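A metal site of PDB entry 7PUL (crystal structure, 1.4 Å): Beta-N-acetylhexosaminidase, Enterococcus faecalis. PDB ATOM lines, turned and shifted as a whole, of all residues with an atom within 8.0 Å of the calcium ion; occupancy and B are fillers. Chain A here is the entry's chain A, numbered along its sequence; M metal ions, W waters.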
ATOM      1  N   ASN A 282      25.134 -15.166  23.061  1.00  0.00           N
ATOM      2  CA  ASN A 282      25.872 -14.104  23.737  1.00  0.00           C
ATOM      3  C   ASN A 282      25.696 -12.865  22.873  1.00  0.00           C
ATOM      4  O   ASN A 282      26.463 -12.590  21.938  1.00  0.00           O
ATOM      5  CB  ASN A 282      27.341 -14.492  23.928  1.00  0.00           C
ATOM      6  CG  ASN A 282      27.517 -15.583  24.977  1.00  0.00           C
ATOM      7  OD1 ASN A 282      26.563 -16.036  25.624  1.00  0.00           O
ATOM      8  ND2 ASN A 282      28.763 -16.022  25.144  1.00  0.00           N
ATOM      9  N   VAL A 283      24.653 -12.091  23.166  1.00  0.00           N
ATOM     10  CA  VAL A 283      24.261 -11.001  22.301  1.00  0.00           C
ATOM     11  C   VAL A 283      24.968  -9.709  22.695  1.00  0.00           C
ATOM     12  O   VAL A 283      25.664  -9.085  21.885  1.00  0.00           O
ATOM     13  CB  VAL A 283      22.738 -10.868  22.279  1.00  0.00           C
ATOM     14  CG1 VAL A 283      22.321  -9.585  21.543  1.00  0.00           C
ATOM     15  CG2 VAL A 283      22.152 -12.102  21.605  1.00  0.00           C
ATOM     16  N   ASP A 284      24.820  -9.332  23.954  1.00  0.00           N
ATOM     17  CA  ASP A 284      25.464  -8.143  24.496  1.00  0.00           C
ATOM     18  C   ASP A 284      26.111  -8.419  25.845  1.00  0.00           C
ATOM     19  O   ASP A 284      26.461  -7.480  26.561  1.00  0.00           O
ATOM     20  CB  ASP A 284      24.444  -7.018  24.619  1.00  0.00           C
ATOM     21  CG  ASP A 284      23.259  -7.392  25.476  1.00  0.00           C
ATOM     22  OD1 ASP A 284      22.281  -6.609  25.496  1.00  0.00           O
ATOM     23  OD2 ASP A 284      23.282  -8.441  26.150  1.00  0.00           O
ATOM     24  N   SER A 285      26.283  -9.695  26.201  1.00  0.00           N
ATOM     25  CA  SER A 285      26.973 -10.067  27.420  1.00  0.00           C
ATOM     26  C   SER A 285      27.685 -11.380  27.165  1.00  0.00           C
ATOM     27  O   SER A 285      27.349 -12.104  26.229  1.00  0.00           O
ATOM     28  CB  SER A 285      26.029 -10.260  28.601  1.00  0.00           C
ATOM     29  OG  SER A 285      25.182 -11.359  28.385  1.00  0.00           O
ATOM     30  N   GLY A 286      28.654 -11.680  28.010  1.00  0.00           N
ATOM     31  CA  GLY A 286      29.412 -12.909  27.888  1.00  0.00           C
ATOM     32  C   GLY A 286      30.596 -12.778  26.946  1.00  0.00           C
ATOM     33  O   GLY A 286      31.058 -11.695  26.590  1.00  0.00           O
ATOM     34  N   TYR A 288      32.679 -13.526  23.354  1.00  0.00           N
ATOM     35  CA  TYR A 288      32.471 -13.601  21.910  1.00  0.00           C
ATOM     36  C   TYR A 288      31.072 -13.117  21.539  1.00  0.00           C
ATOM     37  O   TYR A 288      30.259 -13.819  20.945  1.00  0.00           O
ATOM     38  CB  TYR A 288      32.748 -15.013  21.388  1.00  0.00           C
ATOM     39  CG  TYR A 288      34.170 -15.459  21.622  1.00  0.00           C
ATOM     40  CD1 TYR A 288      35.238 -14.681  21.189  1.00  0.00           C
ATOM     41  CD2 TYR A 288      34.459 -16.666  22.241  1.00  0.00           C
ATOM     42  CE1 TYR A 288      36.557 -15.086  21.376  1.00  0.00           C
ATOM     43  CE2 TYR A 288      35.778 -17.072  22.450  1.00  0.00           C
ATOM     44  CZ  TYR A 288      36.809 -16.290  22.013  1.00  0.00           C
ATOM     45  OH  TYR A 288      38.109 -16.749  22.211  1.00  0.00           O
ATOM     46  N   GLN A 289      30.812 -11.856  21.871  1.00  0.00           N
ATOM     47  CA  GLN A 289      29.504 -11.270  21.714  1.00  0.00           C
ATOM     48  C   GLN A 289      29.210 -10.908  20.265  1.00  0.00           C
ATOM     49  O   GLN A 289      30.111 -10.608  19.465  1.00  0.00           O
ATOM     50  CB  GLN A 289      29.399  -9.999  22.570  1.00  0.00           C
ATOM     51  CG  GLN A 289      29.459 -10.298  24.053  1.00  0.00           C
ATOM     52  CD  GLN A 289      29.424  -9.059  24.876  1.00  0.00           C
ATOM     53  OE1 GLN A 289      28.957  -8.010  24.417  1.00  0.00           O
ATOM     54  NE2 GLN A 289      29.927  -9.143  26.084  1.00  0.00           N
ATOM     55  N   TYR A 290      27.901 -10.828  19.976  1.00  0.00           N
ATOM     56  CA  TYR A 290      27.420 -10.495  18.639  1.00  0.00           C
ATOM     57  C   TYR A 290      27.865  -9.107  18.196  1.00  0.00           C
ATOM     58  O   TYR A 290      28.373  -8.938  17.082  1.00  0.00           O
ATOM     59  CB  TYR A 290      25.902 -10.562  18.680  1.00  0.00           C
ATOM     60  CG  TYR A 290      25.175 -10.195  17.421  1.00  0.00           C
ATOM     61  CD1 TYR A 290      25.286 -10.962  16.280  1.00  0.00           C
ATOM     62  CD2 TYR A 290      24.307  -9.102  17.390  1.00  0.00           C
ATOM     63  CE1 TYR A 290      24.586 -10.665  15.139  1.00  0.00           C
ATOM     64  CE2 TYR A 290      23.590  -8.802  16.253  1.00  0.00           C
ATOM     65  CZ  TYR A 290      23.738  -9.596  15.134  1.00  0.00           C
ATOM     66  OH  TYR A 290      23.039  -9.341  13.960  1.00  0.00           O
ATOM     67  N   ASP A 291      27.625  -8.090  19.038  1.00  0.00           N
ATOM     68  CA  ASP A 291      28.002  -6.736  18.634  1.00  0.00           C
ATOM     69  C   ASP A 291      29.489  -6.630  18.375  1.00  0.00           C
ATOM     70  O   ASP A 291      29.910  -5.977  17.415  1.00  0.00           O
ATOM     71  CB  ASP A 291      27.519  -5.688  19.656  1.00  0.00           C
ATOM     72  CG  ASP A 291      28.171  -5.830  21.019  1.00  0.00           C
ATOM     73  OD1 ASP A 291      28.359  -6.959  21.511  1.00  0.00           O
ATOM     74  OD2 ASP A 291      28.485  -4.793  21.654  1.00  0.00           O
ATOM     75  N   ASP A 292      30.318  -7.286  19.188  1.00  0.00           N
ATOM     76  CA  ASP A 292      31.765  -7.202  18.995  1.00  0.00           C
ATOM     77  C   ASP A 292      32.191  -7.888  17.714  1.00  0.00           C
ATOM     78  O   ASP A 292      33.083  -7.396  16.993  1.00  0.00           O
ATOM     79  CB  ASP A 292      32.491  -7.843  20.172  1.00  0.00           C
ATOM     80  CG  ASP A 292      32.448  -7.003  21.396  1.00  0.00           C
ATOM     81  OD1 ASP A 292      33.485  -6.383  21.731  1.00  0.00           O
ATOM     82  OD2 ASP A 292      31.381  -6.943  22.023  1.00  0.00           O
ATOM     83  N   ALA A 293      31.604  -9.049  17.419  1.00  0.00           N
ATOM     84  CA  ALA A 293      31.949  -9.744  16.200  1.00  0.00           C
ATOM     85  C   ALA A 293      31.673  -8.862  14.996  1.00  0.00           C
ATOM     86  O   ALA A 293      32.533  -8.722  14.113  1.00  0.00           O
ATOM     87  CB  ALA A 293      31.162 -11.064  16.101  1.00  0.00           C
ATOM     88  N   ALA A 295      31.430  -5.554  14.930  1.00  0.00           N
ATOM     89  CA  ALA A 295      32.333  -4.407  14.924  1.00  0.00           C
ATOM     90  C   ALA A 295      33.720  -4.797  14.458  1.00  0.00           C
ATOM     91  O   ALA A 295      34.380  -4.059  13.707  1.00  0.00           O
ATOM     92  CB  ALA A 295      32.423  -3.798  16.318  1.00  0.00           C
HETATM   93 CA    CA M   1      29.659  -6.063  23.378  1.00  0.00          CA
HETATM   94  O   HOH W   1      28.038  -5.299  24.974  1.00  0.00           O
HETATM   95  O   HOH W   2      30.717  -3.968  23.225  1.00  0.00           O
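The nearest printed residue that does not touch the calcium ion is Asp 284 (4.7 Å).
The calcium ion is bound by OE1 of Gln 289, water W2, OD2 of Asp 292, water W1, OD2 of Asp 291 and OD1 of Asp 291.
The calcium ion has six donor atoms within binding distance.
The side-chain amide oxygen (OE1) of Gln 289 sits close to the backbone carbonyl oxygen (O) of Asp 284 (3.3 Å).
NE2 of Gln 289 sits at hydrogen-bond distance from O of Gly 286 (2.8 Å).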
